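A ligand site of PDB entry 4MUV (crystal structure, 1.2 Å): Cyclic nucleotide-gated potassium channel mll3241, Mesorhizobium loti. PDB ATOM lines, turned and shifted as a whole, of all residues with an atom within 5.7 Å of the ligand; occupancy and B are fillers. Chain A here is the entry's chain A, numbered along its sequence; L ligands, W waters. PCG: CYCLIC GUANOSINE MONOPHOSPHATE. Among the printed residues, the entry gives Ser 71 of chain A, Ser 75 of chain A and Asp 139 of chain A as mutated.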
ATOM      1  N   CYS A  50     -13.083  17.155 -14.580  1.00  0.00           N
ATOM      2  CA  CYS A  50     -13.740  15.945 -15.006  1.00  0.00           C
ATOM      3  C   CYS A  50     -12.703  14.859 -15.157  1.00  0.00           C
ATOM      4  O   CYS A  50     -11.516  15.097 -15.291  1.00  0.00           O
ATOM      5  CB  CYS A  50     -14.519  16.172 -16.280  1.00  0.00           C
ATOM      6  SG  CYS A  50     -13.488  16.681 -17.626  1.00  0.00           S
ATOM      7  N   VAL A  69      -5.087  19.305 -19.504  1.00  0.00           N
ATOM      8  CA  VAL A  69      -5.756  18.148 -20.101  1.00  0.00           C
ATOM      9  C   VAL A  69      -4.766  17.007 -20.179  1.00  0.00           C
ATOM     10  O   VAL A  69      -3.729  17.119 -20.837  1.00  0.00           O
ATOM     11  CB  VAL A  69      -6.299  18.467 -21.511  1.00  0.00           C
ATOM     12  CG1 VAL A  69      -7.021  17.239 -22.079  1.00  0.00           C
ATOM     13  CG2 VAL A  69      -7.206  19.706 -21.476  1.00  0.00           C
ATOM     14  N   SER A  71      -3.887  13.950 -21.726  1.00  0.00           N
ATOM     15  CA  SER A  71      -4.162  13.146 -22.913  1.00  0.00           C
ATOM     16  C   SER A  71      -2.804  12.755 -23.457  1.00  0.00           C
ATOM     17  O   SER A  71      -1.807  13.191 -22.892  1.00  0.00           O
ATOM     18  CB  SER A  71      -4.930  13.965 -23.945  1.00  0.00           C
ATOM     19  OG  SER A  71      -4.107  14.967 -24.482  1.00  0.00           O
ATOM     20  N   PRO A  72      -2.758  11.982 -24.558  1.00  0.00           N
ATOM     21  CA  PRO A  72      -1.451  11.560 -25.083  1.00  0.00           C
ATOM     22  C   PRO A  72      -0.583  12.715 -25.531  1.00  0.00           C
ATOM     23  O   PRO A  72       0.630  12.570 -25.635  1.00  0.00           O
ATOM     24  CB  PRO A  72      -1.816  10.654 -26.270  1.00  0.00           C
ATOM     25  CG  PRO A  72      -3.148  10.173 -25.960  1.00  0.00           C
ATOM     26  CD  PRO A  72      -3.860  11.275 -25.235  1.00  0.00           C
ATOM     27  N   ASN A  73      -1.217  13.841 -25.822  1.00  0.00           N
ATOM     28  CA  ASN A  73      -0.505  15.064 -26.148  1.00  0.00           C
ATOM     29  C   ASN A  73      -1.021  16.128 -25.203  1.00  0.00           C
ATOM     30  O   ASN A  73      -1.914  16.897 -25.584  1.00  0.00           O
ATOM     31  CB  ASN A  73      -0.778  15.442 -27.591  1.00  0.00           C
ATOM     32  CG  ASN A  73      -0.252  14.399 -28.555  1.00  0.00           C
ATOM     33  OD1 ASN A  73       0.948  14.311 -28.788  1.00  0.00           O
ATOM     34  ND2 ASN A  73      -1.147  13.586 -29.110  1.00  0.00           N
ATOM     35  N   SER A  75      -2.126  19.152 -22.918  1.00  0.00           N
ATOM     36  CA  SER A  75      -2.243  20.552 -23.297  1.00  0.00           C
ATOM     37  C   SER A  75      -2.834  21.380 -22.158  1.00  0.00           C
ATOM     38  O   SER A  75      -3.370  20.856 -21.186  1.00  0.00           O
ATOM     39  CB  SER A  75      -3.091  20.703 -24.556  1.00  0.00           C
ATOM     40  OG  SER A  75      -4.392  20.200 -24.341  1.00  0.00           O
ATOM     41  N   LEU A  77      -5.373  24.717 -21.492  1.00  0.00           N
ATOM     42  CA  LEU A  77      -6.418  25.545 -22.081  1.00  0.00           C
ATOM     43  C   LEU A  77      -6.625  26.775 -21.214  1.00  0.00           C
ATOM     44  O   LEU A  77      -6.876  26.666 -20.024  1.00  0.00           O
ATOM     45  CB  LEU A  77      -7.726  24.792 -22.211  1.00  0.00           C
ATOM     46  CG  LEU A  77      -7.687  23.469 -22.995  1.00  0.00           C
ATOM     47  CD1 LEU A  77      -9.036  22.785 -22.952  1.00  0.00           C
ATOM     48  CD2 LEU A  77      -7.282  23.715 -24.418  1.00  0.00           C
ATOM     49  N   PHE A  82     -12.544  25.893 -24.426  1.00  0.00           N
ATOM     50  CA  PHE A  82     -13.640  25.134 -23.814  1.00  0.00           C
ATOM     51  C   PHE A  82     -13.306  23.654 -23.820  1.00  0.00           C
ATOM     52  O   PHE A  82     -12.456  23.188 -24.591  1.00  0.00           O
ATOM     53  CB  PHE A  82     -14.989  25.411 -24.498  1.00  0.00           C
ATOM     54  CG  PHE A  82     -14.993  25.136 -25.971  1.00  0.00           C
ATOM     55  CD1 PHE A  82     -15.079  23.844 -26.469  1.00  0.00           C
ATOM     56  CD2 PHE A  82     -14.914  26.181 -26.876  1.00  0.00           C
ATOM     57  CE1 PHE A  82     -15.088  23.590 -27.820  1.00  0.00           C
ATOM     58  CE2 PHE A  82     -14.911  25.938 -28.245  1.00  0.00           C
ATOM     59  CZ  PHE A  82     -15.000  24.627 -28.712  1.00  0.00           C
ATOM     60  N   PHE A  83     -13.937  22.938 -22.909  1.00  0.00           N
ATOM     61  CA  PHE A  83     -13.751  21.488 -22.790  1.00  0.00           C
ATOM     62  C   PHE A  83     -15.002  20.844 -22.224  1.00  0.00           C
ATOM     63  O   PHE A  83     -15.826  21.500 -21.577  1.00  0.00           O
ATOM     64  CB  PHE A  83     -12.514  21.191 -21.939  1.00  0.00           C
ATOM     65  CG  PHE A  83     -12.614  21.624 -20.509  1.00  0.00           C
ATOM     66  CD1 PHE A  83     -12.235  22.899 -20.139  1.00  0.00           C
ATOM     67  CD2 PHE A  83     -13.061  20.758 -19.544  1.00  0.00           C
ATOM     68  CE1 PHE A  83     -12.332  23.292 -18.800  1.00  0.00           C
ATOM     69  CE2 PHE A  83     -13.168  21.158 -18.218  1.00  0.00           C
ATOM     70  CZ  PHE A  83     -12.803  22.409 -17.851  1.00  0.00           C
ATOM     71  N   GLY A  84     -15.132  19.536 -22.454  1.00  0.00           N
ATOM     72  CA  GLY A  84     -16.278  18.761 -22.001  1.00  0.00           C
ATOM     73  C   GLY A  84     -17.346  18.552 -23.048  1.00  0.00           C
ATOM     74  O   GLY A  84     -18.320  17.859 -22.800  1.00  0.00           O
ATOM     75  N   GLU A  85     -17.146  19.145 -24.226  1.00  0.00           N
ATOM     76  CA  GLU A  85     -18.097  18.979 -25.316  1.00  0.00           C
ATOM     77  C   GLU A  85     -18.150  17.557 -25.853  1.00  0.00           C
ATOM     78  O   GLU A  85     -19.181  17.112 -26.323  1.00  0.00           O
ATOM     79  CB  GLU A  85     -17.801  19.936 -26.481  1.00  0.00           C
ATOM     80  CG  GLU A  85     -16.561  19.631 -27.349  1.00  0.00           C
ATOM     81  CD  GLU A  85     -15.246  19.819 -26.576  1.00  0.00           C
ATOM     82  OE1 GLU A  85     -15.200  20.650 -25.639  1.00  0.00           O
ATOM     83  OE2 GLU A  85     -14.261  19.126 -26.910  1.00  0.00           O
ATOM     84  N   MET A  86     -17.056  16.805 -25.771  1.00  0.00           N
ATOM     85  CA  MET A  86     -17.022  15.512 -26.444  1.00  0.00           C
ATOM     86  C   MET A  86     -18.046  14.551 -25.869  1.00  0.00           C
ATOM     87  O   MET A  86     -18.731  13.870 -26.621  1.00  0.00           O
ATOM     88  CB  MET A  86     -15.615  14.920 -26.408  1.00  0.00           C
ATOM     89  CG  MET A  86     -14.631  15.701 -27.268  1.00  0.00           C
ATOM     90  SD  MET A  86     -12.893  15.289 -27.004  1.00  0.00           S
ATOM     91  CE  MET A  86     -12.858  13.678 -27.780  1.00  0.00           C
ATOM     92  N   ALA A  87     -18.153  14.497 -24.549  1.00  0.00           N
ATOM     93  CA  ALA A  87     -19.102  13.567 -23.924  1.00  0.00           C
ATOM     94  C   ALA A  87     -20.534  13.972 -24.250  1.00  0.00           C
ATOM     95  O   ALA A  87     -21.414  13.121 -24.376  1.00  0.00           O
ATOM     96  CB  ALA A  87     -18.918  13.543 -22.444  1.00  0.00           C
ATOM     97  N   LEU A  88     -20.770  15.277 -24.368  1.00  0.00           N
ATOM     98  CA  LEU A  88     -22.116  15.753 -24.684  1.00  0.00           C
ATOM     99  C   LEU A  88     -22.540  15.408 -26.113  1.00  0.00           C
ATOM    100  O   LEU A  88     -23.709  15.117 -26.366  1.00  0.00           O
ATOM    101  CB  LEU A  88     -22.250  17.250 -24.439  1.00  0.00           C
ATOM    102  CG  LEU A  88     -21.919  17.737 -23.039  1.00  0.00           C
ATOM    103  CD1 LEU A  88     -22.175  19.236 -22.900  1.00  0.00           C
ATOM    104  CD2 LEU A  88     -22.700  16.977 -22.002  1.00  0.00           C
ATOM    105  N   PRO A  93     -18.450   8.333 -22.247  1.00  0.00           N
ATOM    106  CA  PRO A  93     -17.823   8.859 -21.039  1.00  0.00           C
ATOM    107  C   PRO A  93     -16.741   9.878 -21.362  1.00  0.00           C
ATOM    108  O   PRO A  93     -16.257   9.964 -22.488  1.00  0.00           O
ATOM    109  CB  PRO A  93     -17.211   7.595 -20.407  1.00  0.00           C
ATOM    110  CG  PRO A  93     -18.079   6.482 -20.935  1.00  0.00           C
ATOM    111  CD  PRO A  93     -18.353   6.864 -22.337  1.00  0.00           C
ATOM    112  N   ARG A  94     -16.366  10.646 -20.364  1.00  0.00           N
ATOM    113  CA  ARG A  94     -15.263  11.573 -20.513  1.00  0.00           C
ATOM    114  C   ARG A  94     -14.051  10.858 -21.085  1.00  0.00           C
ATOM    115  O   ARG A  94     -13.712   9.728 -20.676  1.00  0.00           O
ATOM    116  CB  ARG A  94     -14.859  12.164 -19.170  1.00  0.00           C
ATOM    117  CG  ARG A  94     -15.881  13.010 -18.437  1.00  0.00           C
ATOM    118  CD  ARG A  94     -16.291  14.209 -19.251  1.00  0.00           C
ATOM    119  NE  ARG A  94     -17.153  15.086 -18.466  1.00  0.00           N
ATOM    120  CZ  ARG A  94     -17.833  16.099 -18.963  1.00  0.00           C
ATOM    121  NH1 ARG A  94     -17.797  16.365 -20.257  1.00  0.00           N
ATOM    122  NH2 ARG A  94     -18.566  16.854 -18.149  1.00  0.00           N
ATOM    123  N   SER A  95     -13.371  11.513 -22.001  1.00  0.00           N
ATOM    124  CA  SER A  95     -12.247  10.919 -22.715  1.00  0.00           C
ATOM    125  C   SER A  95     -10.881  11.313 -22.174  1.00  0.00           C
ATOM    126  O   SER A  95      -9.881  10.786 -22.643  1.00  0.00           O
ATOM    127  CB  SER A  95     -12.304  11.258 -24.213  1.00  0.00           C
ATOM    128  OG  SER A  95     -12.095  12.644 -24.441  1.00  0.00           O
ATOM    129  N   ALA A  96     -10.855  12.216 -21.192  1.00  0.00           N
ATOM    130  CA  ALA A  96      -9.612  12.659 -20.593  1.00  0.00           C
ATOM    131  C   ALA A  96      -9.954  13.314 -19.266  1.00  0.00           C
ATOM    132  O   ALA A  96     -11.048  13.844 -19.092  1.00  0.00           O
ATOM    133  CB  ALA A  96      -8.891  13.644 -21.499  1.00  0.00           C
ATOM    134  N   THR A  97      -8.984  13.302 -18.362  1.00  0.00           N
ATOM    135  CA  THR A  97      -9.078  14.018 -17.106  1.00  0.00           C
ATOM    136  C   THR A  97      -8.572  15.454 -17.298  1.00  0.00           C
ATOM    137  O   THR A  97      -7.471  15.677 -17.817  1.00  0.00           O
ATOM    138  CB  THR A  97      -8.294  13.290 -16.021  1.00  0.00           C
ATOM    139  OG1 THR A  97      -8.908  12.003 -15.843  1.00  0.00           O
ATOM    140  CG2 THR A  97      -8.306  14.063 -14.682  1.00  0.00           C
ATOM    141  N   VAL A  98      -9.398  16.407 -16.889  1.00  0.00           N
ATOM    142  CA  VAL A  98      -9.075  17.813 -16.963  1.00  0.00           C
ATOM    143  C   VAL A  98      -9.069  18.341 -15.539  1.00  0.00           C
ATOM    144  O   VAL A  98     -10.003  18.106 -14.788  1.00  0.00           O
ATOM    145  CB  VAL A  98     -10.111  18.587 -17.817  1.00  0.00           C
ATOM    146  CG1 VAL A  98      -9.747  20.062 -17.913  1.00  0.00           C
ATOM    147  CG2 VAL A  98     -10.264  17.949 -19.184  1.00  0.00           C
ATOM    148  N   ARG A 135      -9.703  16.733 -31.498  1.00  0.00           N
ATOM    149  CA  ARG A 135      -9.171  16.200 -30.249  1.00  0.00           C
ATOM    150  C   ARG A 135      -9.020  14.682 -30.334  1.00  0.00           C
ATOM    151  O   ARG A 135      -8.021  14.135 -29.922  1.00  0.00           O
ATOM    152  CB  ARG A 135     -10.013  16.708 -29.063  1.00  0.00           C
ATOM    153  CG  ARG A 135      -9.736  18.194 -28.831  1.00  0.00           C
ATOM    154  CD  ARG A 135     -10.719  18.898 -27.948  1.00  0.00           C
ATOM    155  NE  ARG A 135     -10.268  20.277 -27.749  1.00  0.00           N
ATOM    156  CZ  ARG A 135     -10.869  21.181 -26.977  1.00  0.00           C
ATOM    157  NH1 ARG A 135     -12.013  20.944 -26.397  1.00  0.00           N
ATOM    158  NH2 ARG A 135     -10.299  22.355 -26.832  1.00  0.00           N
ATOM    159  N   ARG A 136     -10.004  14.010 -30.929  1.00  0.00           N
ATOM    160  CA  ARG A 136      -9.873  12.579 -31.229  1.00  0.00           C
ATOM    161  C   ARG A 136      -8.662  12.347 -32.138  1.00  0.00           C
ATOM    162  O   ARG A 136      -7.945  11.353 -31.964  1.00  0.00           O
ATOM    163  CB  ARG A 136     -11.137  12.004 -31.861  1.00  0.00           C
ATOM    164  CG  ARG A 136     -12.339  11.881 -30.926  1.00  0.00           C
ATOM    165  CD  ARG A 136     -12.128  10.928 -29.750  1.00  0.00           C
ATOM    166  NE  ARG A 136     -13.357  10.741 -28.976  1.00  0.00           N
ATOM    167  CZ  ARG A 136     -13.475  10.039 -27.844  1.00  0.00           C
ATOM    168  NH1 ARG A 136     -12.442   9.430 -27.297  1.00  0.00           N
ATOM    169  NH2 ARG A 136     -14.663   9.959 -27.250  1.00  0.00           N
ATOM    170  N   ALA A 138      -5.928  14.217 -32.356  1.00  0.00           N
ATOM    171  CA  ALA A 138      -4.730  14.412 -31.553  1.00  0.00           C
ATOM    172  C   ALA A 138      -4.447  13.163 -30.731  1.00  0.00           C
ATOM    173  O   ALA A 138      -3.295  12.714 -30.633  1.00  0.00           O
ATOM    174  CB  ALA A 138      -4.881  15.637 -30.650  1.00  0.00           C
ATOM    175  N   ASP A 139      -5.492  12.587 -30.164  1.00  0.00           N
ATOM    176  CA  ASP A 139      -5.342  11.383 -29.327  1.00  0.00           C
ATOM    177  C   ASP A 139      -4.816  10.183 -30.098  1.00  0.00           C
ATOM    178  O   ASP A 139      -4.237   9.281 -29.487  1.00  0.00           O
ATOM    179  CB  ASP A 139      -6.685  10.957 -28.741  1.00  0.00           C
ATOM    180  CG  ASP A 139      -7.273  11.935 -27.762  1.00  0.00           C
ATOM    181  OD1 ASP A 139      -6.576  12.882 -27.274  1.00  0.00           O
ATOM    182  OD2 ASP A 139      -8.501  11.785 -27.476  1.00  0.00           O
HETATM  183  PA  PCG L   1     -14.732  15.175 -22.697  1.00  0.00           P
HETATM  184  O1A PCG L   1     -16.208  15.357 -22.438  1.00  0.00           O
HETATM  185  O2A PCG L   1     -14.321  13.863 -23.289  1.00  0.00           O
HETATM  186  O5' PCG L   1     -13.971  15.382 -21.370  1.00  0.00           O
HETATM  187  C5' PCG L   1     -12.633  15.614 -21.380  1.00  0.00           C
HETATM  188  C4' PCG L   1     -12.376  16.810 -22.304  1.00  0.00           C
HETATM  189  O4' PCG L   1     -10.988  17.297 -22.465  1.00  0.00           O
HETATM  190  C3' PCG L   1     -12.809  16.518 -23.582  1.00  0.00           C
HETATM  191  O3' PCG L   1     -14.257  16.346 -23.655  1.00  0.00           O
HETATM  192  C2' PCG L   1     -12.247  17.753 -24.405  1.00  0.00           C
HETATM  193  O2' PCG L   1     -13.229  18.785 -24.413  1.00  0.00           O
HETATM  194  C1' PCG L   1     -11.088  18.135 -23.712  1.00  0.00           C
HETATM  195  N9  PCG L   1      -9.845  18.032 -24.420  1.00  0.00           N
HETATM  196  C8  PCG L   1      -8.998  19.046 -24.775  1.00  0.00           C
HETATM  197  N7  PCG L   1      -7.980  18.610 -25.523  1.00  0.00           N
HETATM  198  C5  PCG L   1      -8.190  17.252 -25.648  1.00  0.00           C
HETATM  199  C6  PCG L   1      -7.445  16.234 -26.335  1.00  0.00           C
HETATM  200  O6  PCG L   1      -6.386  16.415 -26.978  1.00  0.00           O
HETATM  201  N1  PCG L   1      -7.974  14.980 -26.229  1.00  0.00           N
HETATM  202  C2  PCG L   1      -9.155  14.680 -25.573  1.00  0.00           C
HETATM  203  N2  PCG L   1      -9.596  13.408 -25.545  1.00  0.00           N
HETATM  204  N3  PCG L   1      -9.898  15.625 -24.903  1.00  0.00           N
HETATM  205  C4  PCG L   1      -9.352  16.916 -24.986  1.00  0.00           C
HETATM  206  O   HOH W   1      -4.613  17.699 -24.866  1.00  0.00           O
HETATM  207  O   HOH W   2     -16.132  11.956 -24.490  1.00  0.00           O
HETATM  208  O   HOH W   3      -4.234  14.273 -27.363  1.00  0.00           O
HETATM  209  O   HOH W   4      -5.584  18.529 -28.553  1.00  0.00           O
HETATM  210  O   HOH W   5      -6.093  20.492 -26.508  1.00  0.00           O
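OE2 of Glu 85 sits at hydrogen-bond distance from O2' of the ligand, 2.7 Å away.
OD1 of Asp 139 lies within hydrogen-bond range of N1 of the ligand, at 2.7 Å.
O2A of the ligand sits at hydrogen-bond distance from N of Ser 95, 2.8 Å away.
An oxygen (O2A) of the ligand sits at hydrogen-bond distance from the side-chain hydroxyl of Ser 95 (2.8 Å).
O2' of the ligand is in hydrogen-bond range of N of Gly 84, 2.8 Å away.
An oxygen (O1A) of the ligand is in salt-bridge range of the guanidinium group of Arg 94.
The backbone NH of Ala 87 is in hydrogen-bond range of an oxygen (O1A) of the ligand.
NH1 of Arg 135 is in hydrogen-bond range of O2' of the ligand, at 3.2 Å.
The side-chain carboxylate of Glu 85 is in salt-bridge range of the guanidinium group of Arg 135, 2.9 Å away.
The side-chain hydroxyl (OG) of Ser 95 lies close to the side-chain sulfur (SD) of Met 86.
O of Gly 84 lies within hydrogen-bond range of NH1 of Arg 94, at 3.0 Å.
The guanidinium group (NH1) of Arg 135 lies within hydrogen-bond range of the backbone carbonyl oxygen (O) of Phe 82, at 2.9 Å.
N of Val 98 is in hydrogen-bond range of O of Cys 50, 3.0 Å away.
The backbone carbonyl oxygen of Asn 73 is in hydrogen-bond range of the side-chain hydroxyl of Ser 71 (3.1 Å).
The backbone NH (N) of Val 69 sits at hydrogen-bond distance from the backbone carbonyl oxygen (O) of Ser 75 (2.9 Å).
The side-chain sulfur (SD) of Met 86 sits close to a nitrogen (N3) of the ligand (3.7 Å).
Residues that only touch the ligand: Cys 50 (3.99 Å), Val 69 (3.7 Å), Ser 71 (3.7 Å), Phe 83 (3.2 Å), Ala 96 (3.3 Å) and Val 98 (3.4 Å).
Hydrophobic or aromatic side chains within 4 Å of the ligand: Val 69, Phe 83, Met 86, Ala 87 and Val 98.
Of the 24 residues printed, 14 come within 4 Å of the ligand.
Water W5 bridges OG of Ser 75 (2.8 Å) and N7 of the ligand (2.8 Å).
Water W2 lies within hydrogen-bond range of O of Pro 93 (2.8 Å), O2A of the ligand (2.9 Å) and N of Ala 87 (3.2 Å).
Water W1 lies within hydrogen-bond range of OG of Ser 75 (2.6 Å), OG of Ser 71 (2.8 Å), O of Asn 73 (2.9 Å) and O6 of the ligand (3.0 Å).
Water W3 lies within hydrogen-bond range of OD1 of Asp 139 (2.7 Å), OG of Ser 71 (3.0 Å), O6 of the ligand (3.1 Å) and N of Asn 73 (3.4 Å).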
